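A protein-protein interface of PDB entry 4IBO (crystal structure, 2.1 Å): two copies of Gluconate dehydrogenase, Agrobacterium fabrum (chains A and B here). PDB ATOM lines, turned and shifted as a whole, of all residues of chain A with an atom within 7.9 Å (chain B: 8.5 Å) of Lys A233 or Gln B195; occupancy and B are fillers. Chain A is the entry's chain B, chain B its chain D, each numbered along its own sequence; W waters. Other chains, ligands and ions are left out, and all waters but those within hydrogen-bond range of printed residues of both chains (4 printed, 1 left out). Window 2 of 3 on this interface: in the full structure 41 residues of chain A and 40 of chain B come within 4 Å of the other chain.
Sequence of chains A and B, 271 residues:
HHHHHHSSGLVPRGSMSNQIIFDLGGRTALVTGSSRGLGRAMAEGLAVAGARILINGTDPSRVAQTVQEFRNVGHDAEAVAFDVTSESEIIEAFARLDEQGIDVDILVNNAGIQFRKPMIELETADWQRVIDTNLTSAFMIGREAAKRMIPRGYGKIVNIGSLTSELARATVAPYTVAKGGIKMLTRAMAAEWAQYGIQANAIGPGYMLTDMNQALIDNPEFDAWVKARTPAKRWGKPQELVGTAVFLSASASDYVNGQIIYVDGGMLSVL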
ATOM      1  N   ASP A 223       2.350  31.204   3.237  1.00  0.00           N
ATOM      2  CA  ASP A 223       1.967  29.853   2.853  1.00  0.00           C
ATOM      3  C   ASP A 223       2.778  28.820   3.629  1.00  0.00           C
ATOM      4  O   ASP A 223       2.216  27.893   4.215  1.00  0.00           O
ATOM      5  CB  ASP A 223       2.165  29.653   1.347  1.00  0.00           C
ATOM      6  CG  ASP A 223       1.692  28.290   0.873  1.00  0.00           C
ATOM      7  OD1 ASP A 223       0.655  27.801   1.376  1.00  0.00           O
ATOM      8  OD2 ASP A 223       2.355  27.703  -0.006  1.00  0.00           O
ATOM      9  N   ALA A 224       4.098  28.993   3.644  1.00  0.00           N
ATOM     10  CA  ALA A 224       4.976  28.091   4.378  1.00  0.00           C
ATOM     11  C   ALA A 224       4.652  28.086   5.873  1.00  0.00           C
ATOM     12  O   ALA A 224       4.678  27.037   6.509  1.00  0.00           O
ATOM     13  CB  ALA A 224       6.449  28.453   4.143  1.00  0.00           C
ATOM     14  N   TRP A 225       4.356  29.256   6.433  1.00  0.00           N
ATOM     15  CA  TRP A 225       4.014  29.349   7.853  1.00  0.00           C
ATOM     16  C   TRP A 225       2.731  28.575   8.168  1.00  0.00           C
ATOM     17  O   TRP A 225       2.704  27.780   9.104  1.00  0.00           O
ATOM     18  CB  TRP A 225       3.898  30.812   8.296  1.00  0.00           C
ATOM     19  CG  TRP A 225       3.334  30.985   9.680  1.00  0.00           C
ATOM     20  CD1 TRP A 225       4.020  30.947  10.868  1.00  0.00           C
ATOM     21  CD2 TRP A 225       1.967  31.239  10.016  1.00  0.00           C
ATOM     22  NE1 TRP A 225       3.154  31.153  11.919  1.00  0.00           N
ATOM     23  CE2 TRP A 225       1.889  31.335  11.422  1.00  0.00           C
ATOM     24  CE3 TRP A 225       0.796  31.390   9.262  1.00  0.00           C
ATOM     25  CZ2 TRP A 225       0.689  31.578  12.087  1.00  0.00           C
ATOM     26  CZ3 TRP A 225      -0.396  31.628   9.921  1.00  0.00           C
ATOM     27  CH2 TRP A 225      -0.439  31.726  11.318  1.00  0.00           C
ATOM     28  N   VAL A 226       1.677  28.789   7.386  1.00  0.00           N
ATOM     29  CA  VAL A 226       0.441  28.033   7.585  1.00  0.00           C
ATOM     30  C   VAL A 226       0.715  26.528   7.649  1.00  0.00           C
ATOM     31  O   VAL A 226       0.301  25.854   8.597  1.00  0.00           O
ATOM     32  CB  VAL A 226      -0.596  28.316   6.475  1.00  0.00           C
ATOM     33  CG1 VAL A 226      -1.767  27.358   6.585  1.00  0.00           C
ATOM     34  CG2 VAL A 226      -1.078  29.754   6.554  1.00  0.00           C
ATOM     35  N   LYS A 227       1.433  26.016   6.651  1.00  0.00           N
ATOM     36  CA  LYS A 227       1.717  24.587   6.555  1.00  0.00           C
ATOM     37  C   LYS A 227       2.583  24.066   7.702  1.00  0.00           C
ATOM     38  O   LYS A 227       2.421  22.924   8.128  1.00  0.00           O
ATOM     39  CB  LYS A 227       2.362  24.257   5.204  1.00  0.00           C
ATOM     40  CG  LYS A 227       1.397  24.384   4.020  1.00  0.00           C
ATOM     41  CD  LYS A 227       2.146  24.284   2.686  1.00  0.00           C
ATOM     42  CE  LYS A 227       1.230  24.634   1.507  1.00  0.00           C
ATOM     43  NZ  LYS A 227       1.996  24.780   0.231  1.00  0.00           N
ATOM     44  N   ALA A 228       3.497  24.894   8.200  1.00  0.00           N
ATOM     45  CA  ALA A 228       4.333  24.499   9.337  1.00  0.00           C
ATOM     46  C   ALA A 228       3.631  24.682  10.690  1.00  0.00           C
ATOM     47  O   ALA A 228       3.962  23.996  11.661  1.00  0.00           O
ATOM     48  CB  ALA A 228       5.646  25.251   9.321  1.00  0.00           C
ATOM     49  N   ARG A 229       2.662  25.596  10.752  1.00  0.00           N
ATOM     50  CA  ARG A 229       2.008  25.950  12.018  1.00  0.00           C
ATOM     51  C   ARG A 229       0.810  25.039  12.297  1.00  0.00           C
ATOM     52  O   ARG A 229       0.406  24.853  13.450  1.00  0.00           O
ATOM     53  CB  ARG A 229       1.576  27.428  11.991  1.00  0.00           C
ATOM     54  CG  ARG A 229       0.817  27.926  13.223  1.00  0.00           C
ATOM     55  CD  ARG A 229       1.667  27.825  14.502  1.00  0.00           C
ATOM     56  NE  ARG A 229       0.964  28.341  15.679  1.00  0.00           N
ATOM     57  CZ  ARG A 229      -0.007  27.691  16.317  1.00  0.00           C
ATOM     58  NH1 ARG A 229      -0.400  26.496  15.890  1.00  0.00           N
ATOM     59  NH2 ARG A 229      -0.590  28.234  17.383  1.00  0.00           N
ATOM     60  N   THR A 230       0.259  24.468  11.229  1.00  0.00           N
ATOM     61  CA  THR A 230      -0.910  23.596  11.296  1.00  0.00           C
ATOM     62  C   THR A 230      -0.454  22.143  11.366  1.00  0.00           C
ATOM     63  O   THR A 230       0.304  21.688  10.505  1.00  0.00           O
ATOM     64  CB  THR A 230      -1.783  23.761  10.029  1.00  0.00           C
ATOM     65  OG1 THR A 230      -2.019  25.154   9.787  1.00  0.00           O
ATOM     66  CG2 THR A 230      -3.124  23.048  10.188  1.00  0.00           C
ATOM     67  N   PRO A 231      -0.913  21.406  12.391  1.00  0.00           N
ATOM     68  CA  PRO A 231      -0.547  19.990  12.540  1.00  0.00           C
ATOM     69  C   PRO A 231      -0.917  19.162  11.303  1.00  0.00           C
ATOM     70  O   PRO A 231      -0.185  18.241  10.942  1.00  0.00           O
ATOM     71  CB  PRO A 231      -1.375  19.547  13.748  1.00  0.00           C
ATOM     72  CG  PRO A 231      -1.517  20.801  14.570  1.00  0.00           C
ATOM     73  CD  PRO A 231      -1.675  21.906  13.551  1.00  0.00           C
ATOM     74  N   ALA A 232      -2.032  19.498  10.655  1.00  0.00           N
ATOM     75  CA  ALA A 232      -2.448  18.783   9.447  1.00  0.00           C
ATOM     76  C   ALA A 232      -1.550  19.134   8.263  1.00  0.00           C
ATOM     77  O   ALA A 232      -1.642  18.515   7.202  1.00  0.00           O
ATOM     78  CB  ALA A 232      -3.901  19.092   9.120  1.00  0.00           C
ATOM     79  N   LYS A 233      -0.698  20.142   8.451  1.00  0.00           N
ATOM     80  CA  LYS A 233       0.243  20.595   7.419  1.00  0.00           C
ATOM     81  C   LYS A 233      -0.404  21.021   6.092  1.00  0.00           C
ATOM     82  O   LYS A 233       0.174  20.823   5.024  1.00  0.00           O
ATOM     83  CB  LYS A 233       1.328  19.538   7.172  1.00  0.00           C
ATOM     84  CG  LYS A 233       2.214  19.283   8.391  1.00  0.00           C
ATOM     85  CD  LYS A 233       3.457  18.489   8.011  1.00  0.00           C
ATOM     86  CE  LYS A 233       4.428  18.407   9.181  1.00  0.00           C
ATOM     87  NZ  LYS A 233       4.889  19.755   9.621  1.00  0.00           N
ATOM     88  N   ARG A 234      -1.587  21.625   6.161  1.00  0.00           N
ATOM     89  CA  ARG A 234      -2.273  22.069   4.951  1.00  0.00           C
ATOM     90  C   ARG A 234      -3.330  23.125   5.270  1.00  0.00           C
ATOM     91  O   ARG A 234      -3.801  23.229   6.409  1.00  0.00           O
ATOM     92  CB  ARG A 234      -2.952  20.881   4.255  1.00  0.00           C
ATOM     93  CG  ARG A 234      -4.128  20.277   5.049  1.00  0.00           C
ATOM     94  CD  ARG A 234      -4.744  19.096   4.282  1.00  0.00           C
ATOM     95  NE  ARG A 234      -5.866  18.460   4.973  1.00  0.00           N
ATOM     96  CZ  ARG A 234      -7.131  18.872   4.885  1.00  0.00           C
ATOM     97  NH1 ARG A 234      -7.437  19.943   4.158  1.00  0.00           N
ATOM     98  NH2 ARG A 234      -8.092  18.221   5.532  1.00  0.00           N
ATOM     99  N   TRP A 235      -3.702  23.901   4.256  1.00  0.00           N
ATOM    100  CA  TRP A 235      -4.854  24.792   4.351  1.00  0.00           C
ATOM    101  C   TRP A 235      -6.132  23.960   4.291  1.00  0.00           C
ATOM    102  O   TRP A 235      -6.137  22.850   3.747  1.00  0.00           O
ATOM    103  CB  TRP A 235      -4.861  25.757   3.166  1.00  0.00           C
ATOM    104  CG  TRP A 235      -3.728  26.739   3.124  1.00  0.00           C
ATOM    105  CD1 TRP A 235      -2.406  26.470   2.888  1.00  0.00           C
ATOM    106  CD2 TRP A 235      -3.827  28.159   3.276  1.00  0.00           C
ATOM    107  NE1 TRP A 235      -1.676  27.640   2.907  1.00  0.00           N
ATOM    108  CE2 TRP A 235      -2.527  28.691   3.144  1.00  0.00           C
ATOM    109  CE3 TRP A 235      -4.893  29.034   3.520  1.00  0.00           C
ATOM    110  CZ2 TRP A 235      -2.263  30.060   3.248  1.00  0.00           C
ATOM    111  CZ3 TRP A 235      -4.628  30.394   3.629  1.00  0.00           C
ATOM    112  CH2 TRP A 235      -3.324  30.891   3.491  1.00  0.00           C
ATOM    113  N   GLY A 236      -7.224  24.500   4.825  1.00  0.00           N
ATOM    114  CA  GLY A 236      -8.522  23.867   4.671  1.00  0.00           C
ATOM    115  C   GLY A 236      -9.202  24.318   3.383  1.00  0.00           C
ATOM    116  O   GLY A 236      -8.933  25.416   2.876  1.00  0.00           O
ATOM    117  N   ASP A 264      -9.632  23.762  11.759  1.00  0.00           N
ATOM    118  CA  ASP A 264      -8.354  24.426  11.557  1.00  0.00           C
ATOM    119  C   ASP A 264      -7.175  23.480  11.439  1.00  0.00           C
ATOM    120  O   ASP A 264      -6.036  23.904  11.603  1.00  0.00           O
ATOM    121  CB  ASP A 264      -8.087  25.436  12.693  1.00  0.00           C
ATOM    122  CG  ASP A 264      -7.801  24.766  14.044  1.00  0.00           C
ATOM    123  OD1 ASP A 264      -8.025  23.541  14.196  1.00  0.00           O
ATOM    124  OD2 ASP A 264      -7.358  25.480  14.974  1.00  0.00           O
ATOM    125  N   GLY A 265      -7.442  22.205  11.168  1.00  0.00           N
ATOM    126  CA  GLY A 265      -6.372  21.227  11.043  1.00  0.00           C
ATOM    127  C   GLY A 265      -5.534  21.053  12.298  1.00  0.00           C
ATOM    128  O   GLY A 265      -4.416  20.509  12.233  1.00  0.00           O
ATOM    129  N   GLY A 266      -6.060  21.512  13.439  1.00  0.00           N
ATOM    130  CA  GLY A 266      -5.372  21.355  14.720  1.00  0.00           C
ATOM    131  C   GLY A 266      -4.595  22.574  15.187  1.00  0.00           C
ATOM    132  O   GLY A 266      -3.967  22.570  16.257  1.00  0.00           O
ATOM    133  N   ILE B 150      -1.458   5.196  10.960  1.00  0.00           N
ATOM    134  CA  ILE B 150      -0.434   5.992  10.276  1.00  0.00           C
ATOM    135  C   ILE B 150      -0.037   5.477   8.873  1.00  0.00           C
ATOM    136  O   ILE B 150      -0.117   6.235   7.901  1.00  0.00           O
ATOM    137  CB  ILE B 150       0.792   6.261  11.188  1.00  0.00           C
ATOM    138  CG1 ILE B 150       0.414   7.267  12.275  1.00  0.00           C
ATOM    139  CG2 ILE B 150       1.980   6.767  10.381  1.00  0.00           C
ATOM    140  CD1 ILE B 150       1.465   7.414  13.350  1.00  0.00           C
ATOM    141  N   GLY B 153      -2.757   6.074   6.367  1.00  0.00           N
ATOM    142  CA  GLY B 153      -2.913   7.474   5.992  1.00  0.00           C
ATOM    143  C   GLY B 153      -4.242   8.128   6.344  1.00  0.00           C
ATOM    144  O   GLY B 153      -4.556   9.222   5.857  1.00  0.00           O
ATOM    145  N   TYR B 154      -5.023   7.459   7.188  1.00  0.00           N
ATOM    146  CA  TYR B 154      -6.307   7.987   7.638  1.00  0.00           C
ATOM    147  C   TYR B 154      -6.710   7.297   8.925  1.00  0.00           C
ATOM    148  O   TYR B 154      -6.268   6.180   9.214  1.00  0.00           O
ATOM    149  CB  TYR B 154      -7.399   7.796   6.579  1.00  0.00           C
ATOM    150  CG  TYR B 154      -7.591   6.359   6.140  1.00  0.00           C
ATOM    151  CD1 TYR B 154      -6.785   5.806   5.150  1.00  0.00           C
ATOM    152  CD2 TYR B 154      -8.580   5.557   6.705  1.00  0.00           C
ATOM    153  CE1 TYR B 154      -6.946   4.493   4.734  1.00  0.00           C
ATOM    154  CE2 TYR B 154      -8.750   4.235   6.299  1.00  0.00           C
ATOM    155  CZ  TYR B 154      -7.926   3.712   5.308  1.00  0.00           C
ATOM    156  OH  TYR B 154      -8.080   2.407   4.886  1.00  0.00           O
ATOM    157  N   MET B 189      -2.267  14.097  20.640  1.00  0.00           N
ATOM    158  CA  MET B 189      -2.482  13.171  19.526  1.00  0.00           C
ATOM    159  C   MET B 189      -2.606  13.912  18.204  1.00  0.00           C
ATOM    160  O   MET B 189      -2.017  13.500  17.201  1.00  0.00           O
ATOM    161  CB  MET B 189      -3.735  12.323  19.748  1.00  0.00           C
ATOM    162  CG  MET B 189      -3.628  11.290  20.859  1.00  0.00           C
ATOM    163  SD  MET B 189      -5.191  10.403  21.010  1.00  0.00           S
ATOM    164  CE  MET B 189      -4.697   9.112  22.163  1.00  0.00           C
ATOM    165  N   ALA B 190      -3.370  15.004  18.204  1.00  0.00           N
ATOM    166  CA  ALA B 190      -3.464  15.863  17.020  1.00  0.00           C
ATOM    167  C   ALA B 190      -2.081  16.396  16.634  1.00  0.00           C
ATOM    168  O   ALA B 190      -1.701  16.355  15.466  1.00  0.00           O
ATOM    169  CB  ALA B 190      -4.433  17.013  17.270  1.00  0.00           C
ATOM    170  N   ALA B 191      -1.330  16.881  17.623  1.00  0.00           N
ATOM    171  CA  ALA B 191       0.029  17.390  17.393  1.00  0.00           C
ATOM    172  C   ALA B 191       0.921  16.405  16.635  1.00  0.00           C
ATOM    173  O   ALA B 191       1.679  16.802  15.744  1.00  0.00           O
ATOM    174  CB  ALA B 191       0.685  17.757  18.717  1.00  0.00           C
ATOM    175  N   GLU B 192       0.837  15.124  16.993  1.00  0.00           N
ATOM    176  CA  GLU B 192       1.735  14.116  16.433  1.00  0.00           C
ATOM    177  C   GLU B 192       1.177  13.394  15.209  1.00  0.00           C
ATOM    178  O   GLU B 192       1.940  12.983  14.326  1.00  0.00           O
ATOM    179  CB  GLU B 192       2.134  13.092  17.507  1.00  0.00           C
ATOM    180  CG  GLU B 192       2.908  13.707  18.679  1.00  0.00           C
ATOM    181  CD  GLU B 192       3.492  12.676  19.632  1.00  0.00           C
ATOM    182  OE1 GLU B 192       3.444  11.460  19.325  1.00  0.00           O
ATOM    183  OE2 GLU B 192       4.004  13.086  20.695  1.00  0.00           O
ATOM    184  N   TRP B 193      -0.146  13.233  15.153  1.00  0.00           N
ATOM    185  CA  TRP B 193      -0.741  12.370  14.135  1.00  0.00           C
ATOM    186  C   TRP B 193      -1.525  13.074  13.030  1.00  0.00           C
ATOM    187  O   TRP B 193      -1.722  12.491  11.965  1.00  0.00           O
ATOM    188  CB  TRP B 193      -1.587  11.278  14.796  1.00  0.00           C
ATOM    189  CG  TRP B 193      -0.802  10.481  15.788  1.00  0.00           C
ATOM    190  CD1 TRP B 193       0.555  10.269  15.791  1.00  0.00           C
ATOM    191  CD2 TRP B 193      -1.315   9.809  16.943  1.00  0.00           C
ATOM    192  NE1 TRP B 193       0.907   9.496  16.873  1.00  0.00           N
ATOM    193  CE2 TRP B 193      -0.225   9.200  17.594  1.00  0.00           C
ATOM    194  CE3 TRP B 193      -2.595   9.663  17.488  1.00  0.00           C
ATOM    195  CZ2 TRP B 193      -0.377   8.450  18.769  1.00  0.00           C
ATOM    196  CZ3 TRP B 193      -2.741   8.919  18.645  1.00  0.00           C
ATOM    197  CH2 TRP B 193      -1.641   8.325  19.273  1.00  0.00           C
ATOM    198  N   ALA B 194      -1.950  14.317  13.262  1.00  0.00           N
ATOM    199  CA  ALA B 194      -2.722  15.039  12.240  1.00  0.00           C
ATOM    200  C   ALA B 194      -2.026  15.005  10.879  1.00  0.00           C
ATOM    201  O   ALA B 194      -2.679  14.863   9.850  1.00  0.00           O
ATOM    202  CB  ALA B 194      -2.983  16.480  12.664  1.00  0.00           C
ATOM    203  N   GLN B 195      -0.698  15.099  10.888  1.00  0.00           N
ATOM    204  CA  GLN B 195       0.074  15.141   9.643  1.00  0.00           C
ATOM    205  C   GLN B 195      -0.041  13.849   8.836  1.00  0.00           C
ATOM    206  O   GLN B 195       0.148  13.853   7.618  1.00  0.00           O
ATOM    207  CB  GLN B 195       1.553  15.454   9.935  1.00  0.00           C
ATOM    208  CG  GLN B 195       2.290  14.344  10.671  1.00  0.00           C
ATOM    209  CD  GLN B 195       3.682  14.758  11.108  1.00  0.00           C
ATOM    210  OE1 GLN B 195       4.557  15.021  10.281  1.00  0.00           O
ATOM    211  NE2 GLN B 195       3.892  14.820  12.417  1.00  0.00           N
ATOM    212  N   TYR B 196      -0.349  12.745   9.512  1.00  0.00           N
ATOM    213  CA  TYR B 196      -0.487  11.466   8.827  1.00  0.00           C
ATOM    214  C   TYR B 196      -1.930  11.209   8.407  1.00  0.00           C
ATOM    215  O   TYR B 196      -2.267  10.110   7.974  1.00  0.00           O
ATOM    216  CB  TYR B 196       0.038  10.329   9.702  1.00  0.00           C
ATOM    217  CG  TYR B 196       1.483  10.514  10.095  1.00  0.00           C
ATOM    218  CD1 TYR B 196       2.476  10.585   9.127  1.00  0.00           C
ATOM    219  CD2 TYR B 196       1.856  10.632  11.431  1.00  0.00           C
ATOM    220  CE1 TYR B 196       3.798  10.760   9.477  1.00  0.00           C
ATOM    221  CE2 TYR B 196       3.186  10.806  11.791  1.00  0.00           C
ATOM    222  CZ  TYR B 196       4.148  10.868  10.806  1.00  0.00           C
ATOM    223  OH  TYR B 196       5.466  11.040  11.142  1.00  0.00           O
ATOM    224  N   GLY B 197      -2.781  12.225   8.536  1.00  0.00           N
ATOM    225  CA  GLY B 197      -4.169  12.105   8.111  1.00  0.00           C
ATOM    226  C   GLY B 197      -5.101  11.528   9.166  1.00  0.00           C
ATOM    227  O   GLY B 197      -6.177  11.013   8.854  1.00  0.00           O
ATOM    228  N   ILE B 198      -4.689  11.613  10.423  1.00  0.00           N
ATOM    229  CA  ILE B 198      -5.505  11.128  11.531  1.00  0.00           C
ATOM    230  C   ILE B 198      -6.125  12.307  12.276  1.00  0.00           C
ATOM    231  O   ILE B 198      -5.417  13.248  12.625  1.00  0.00           O
ATOM    232  CB  ILE B 198      -4.635  10.339  12.512  1.00  0.00           C
ATOM    233  CG1 ILE B 198      -4.171   9.033  11.871  1.00  0.00           C
ATOM    234  CG2 ILE B 198      -5.370  10.076  13.819  1.00  0.00           C
ATOM    235  CD1 ILE B 198      -3.044   8.383  12.632  1.00  0.00           C
ATOM    236  N   GLN B 199      -7.435  12.266  12.514  1.00  0.00           N
ATOM    237  CA  GLN B 199      -8.077  13.299  13.329  1.00  0.00           C
ATOM    238  C   GLN B 199      -8.411  12.796  14.727  1.00  0.00           C
ATOM    239  O   GLN B 199      -9.217  11.869  14.904  1.00  0.00           O
ATOM    240  CB  GLN B 199      -9.339  13.848  12.664  1.00  0.00           C
ATOM    241  CG  GLN B 199      -9.058  14.618  11.380  1.00  0.00           C
ATOM    242  CD  GLN B 199      -8.836  13.685  10.210  1.00  0.00           C
ATOM    243  OE1 GLN B 199      -9.720  12.891   9.858  1.00  0.00           O
ATOM    244  NE2 GLN B 199      -7.650  13.757   9.607  1.00  0.00           N
ATOM    245  N   TYR B 255     -11.033  18.116   8.651  1.00  0.00           N
ATOM    246  CA  TYR B 255     -10.132  19.217   8.980  1.00  0.00           C
ATOM    247  C   TYR B 255     -10.339  19.688  10.416  1.00  0.00           C
ATOM    248  O   TYR B 255      -9.868  20.755  10.795  1.00  0.00           O
ATOM    249  CB  TYR B 255     -10.323  20.386   8.004  1.00  0.00           C
ATOM    250  CG  TYR B 255      -9.153  21.356   7.955  1.00  0.00           C
ATOM    251  CD1 TYR B 255      -7.861  20.911   7.689  1.00  0.00           C
ATOM    252  CD2 TYR B 255      -9.346  22.718   8.156  1.00  0.00           C
ATOM    253  CE1 TYR B 255      -6.788  21.802   7.633  1.00  0.00           C
ATOM    254  CE2 TYR B 255      -8.286  23.614   8.109  1.00  0.00           C
ATOM    255  CZ  TYR B 255      -7.013  23.151   7.841  1.00  0.00           C
ATOM    256  OH  TYR B 255      -5.968  24.047   7.790  1.00  0.00           O
ATOM    257  N   ASN B 257      -9.410  18.951  14.208  1.00  0.00           N
ATOM    258  CA  ASN B 257      -8.354  18.214  14.906  1.00  0.00           C
ATOM    259  C   ASN B 257      -8.068  18.851  16.250  1.00  0.00           C
ATOM    260  O   ASN B 257      -7.925  20.078  16.336  1.00  0.00           O
ATOM    261  CB  ASN B 257      -7.066  18.203  14.065  1.00  0.00           C
ATOM    262  CG  ASN B 257      -6.524  16.799  13.818  1.00  0.00           C
ATOM    263  OD1 ASN B 257      -6.304  16.017  14.760  1.00  0.00           O
ATOM    264  ND2 ASN B 257      -6.290  16.474  12.545  1.00  0.00           N
HETATM  265  O   HOH W   1      -6.005  26.266   9.609  1.00  0.00           O
HETATM  266  O   HOH W   2       0.782  16.215  12.948  1.00  0.00           O
HETATM  267  O   HOH W   3      -7.699  15.370   6.695  1.00  0.00           O
HETATM  268  O   HOH W   4      -9.898  21.848  14.348  1.00  0.00           O
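Printed residues of chain A that touch a printed residue of chain B: Thr A230, Pro A231, Ala A232, Lys A233, Arg A234, Trp A235, Gly A236, Asp A264, Gly A265 and Gly A266.
Hydrophobic or aromatic side chains of chain A within 4 Å of the printed part of chain B: Pro A231.
Along chain A the printed residues that touch a printed residue of chain B span positions 230 to 266.
Of the 16 printed residues of chain B, 5 touch a printed residue of chain A.
Printed residues of chain B that touch a printed residue of chain A: Ala B190, Ala B194, Gln B195, Tyr B255 and Asn B257.
Hydrophobic or aromatic side chains of chain B within 4 Å of the printed part of chain A: Ala B194 and Tyr B255.
Along chain B the printed residues that touch a printed residue of chain A span positions 190 to 257.
Among the printed residues, no Asp or Glu carboxylate lies within 4 Å of a Lys or Arg side-chain nitrogen of the other chain.
Among the printed residues, pairs that only touch across the chains: Thr A230 with Tyr B255, Pro A231 with Ala B190, Pro A231 with Ala B194, Ala A232 with Ala B194, Lys A233 with Gln B195, Trp A235 with Tyr B255, Gly A265 with Asn B257 and Gly A266 with Asn B257.
Lys A233 touches just one residue of chain B: Gln B195.
Gln B195 touches just these residues of chain A: Pro A231 (3.2 Å) and Lys A233 (3.6 Å).
Of chain B, only Ala B194 (3.7 Å) comes within 4 Å of Ala A232.
Ala B194 touches just these residues of chain A: Pro A231 (3.6 Å) and Ala A232 (3.7 Å).
Of the printed residues of chain A, Ala B190 touches Pro A231.
Of the printed residues of chain B, Thr A230 touches Tyr B255.
Of the printed residues of chain A, Tyr B255 touches Thr A230, Arg A234, Trp A235, Gly A236, Asp A264 and Gly A265.
Val A226 touches none of the printed residues of chain B.
The nearest residue of chain B that does not touch Lys A233 is Ala B194 (5.8 Å).
The nearest printed residue of chain B that does not touch Arg A234 is Gln B199 (6.1 Å).
Water W4 lies within hydrogen-bond range of the side-chain carboxylate of Asp A264 (2.5 Å) and the backbone NH of Asn B257 (2.9 Å).
Water W2 lies within hydrogen-bond range of the backbone NH of Gln B195 (2.8 Å), the backbone carbonyl oxygen of Ala B191 (3.0 Å), the backbone carbonyl oxygen of Pro A231 (3.0 Å) and the backbone NH of Ala B194 (3.3 Å).
Water W1 bridges OH of Tyr B255 (2.9 Å) and O of Asp A264 (3.1 Å).
Water W3 lies within hydrogen-bond range of the guanidinium group (NH2) of Arg A234 and the side-chain amide nitrogen (NE2) of Gln B199.
OD1 of Asp A223 lies within hydrogen-bond range of NE1 of Trp A235.
OG1 of Thr A230 is in hydrogen-bond range of O of Val A226.
O of Gly A265 lies within hydrogen-bond range of N of Ala A232, at 3.0 Å.
The side-chain carboxylate of Asp A264 lies within hydrogen-bond range of the backbone NH of Gly A266, 2.9 Å away.
O of Glu B192 sits at hydrogen-bond distance from NE2 of Gln B195 (3.3 Å).
The side-chain amide nitrogen of Asn B257 lies within hydrogen-bond range of the backbone carbonyl oxygen of Ile B198 (3.3 Å).
N of Gln B195 lies within hydrogen-bond range of O of Pro A231 (3.2 Å).
The backbone carbonyl oxygen (O) of Arg A234 lies within hydrogen-bond range of the side-chain hydroxyl (OH) of Tyr B255 (2.7 Å).
The backbone NH of Gly A236 sits at hydrogen-bond distance from the side-chain hydroxyl of Tyr B255 (3.3 Å).
N of Asp A264 lies within hydrogen-bond range of O of Tyr B255, 3.2 Å away.
N of Gly A265 is in hydrogen-bond range of O of Tyr B255, at 2.9 Å.
No position is printed for both chains.
Of the 13 pairs that touch across the chains among the printed residues, none has its exchanged pair printed and touching as well.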
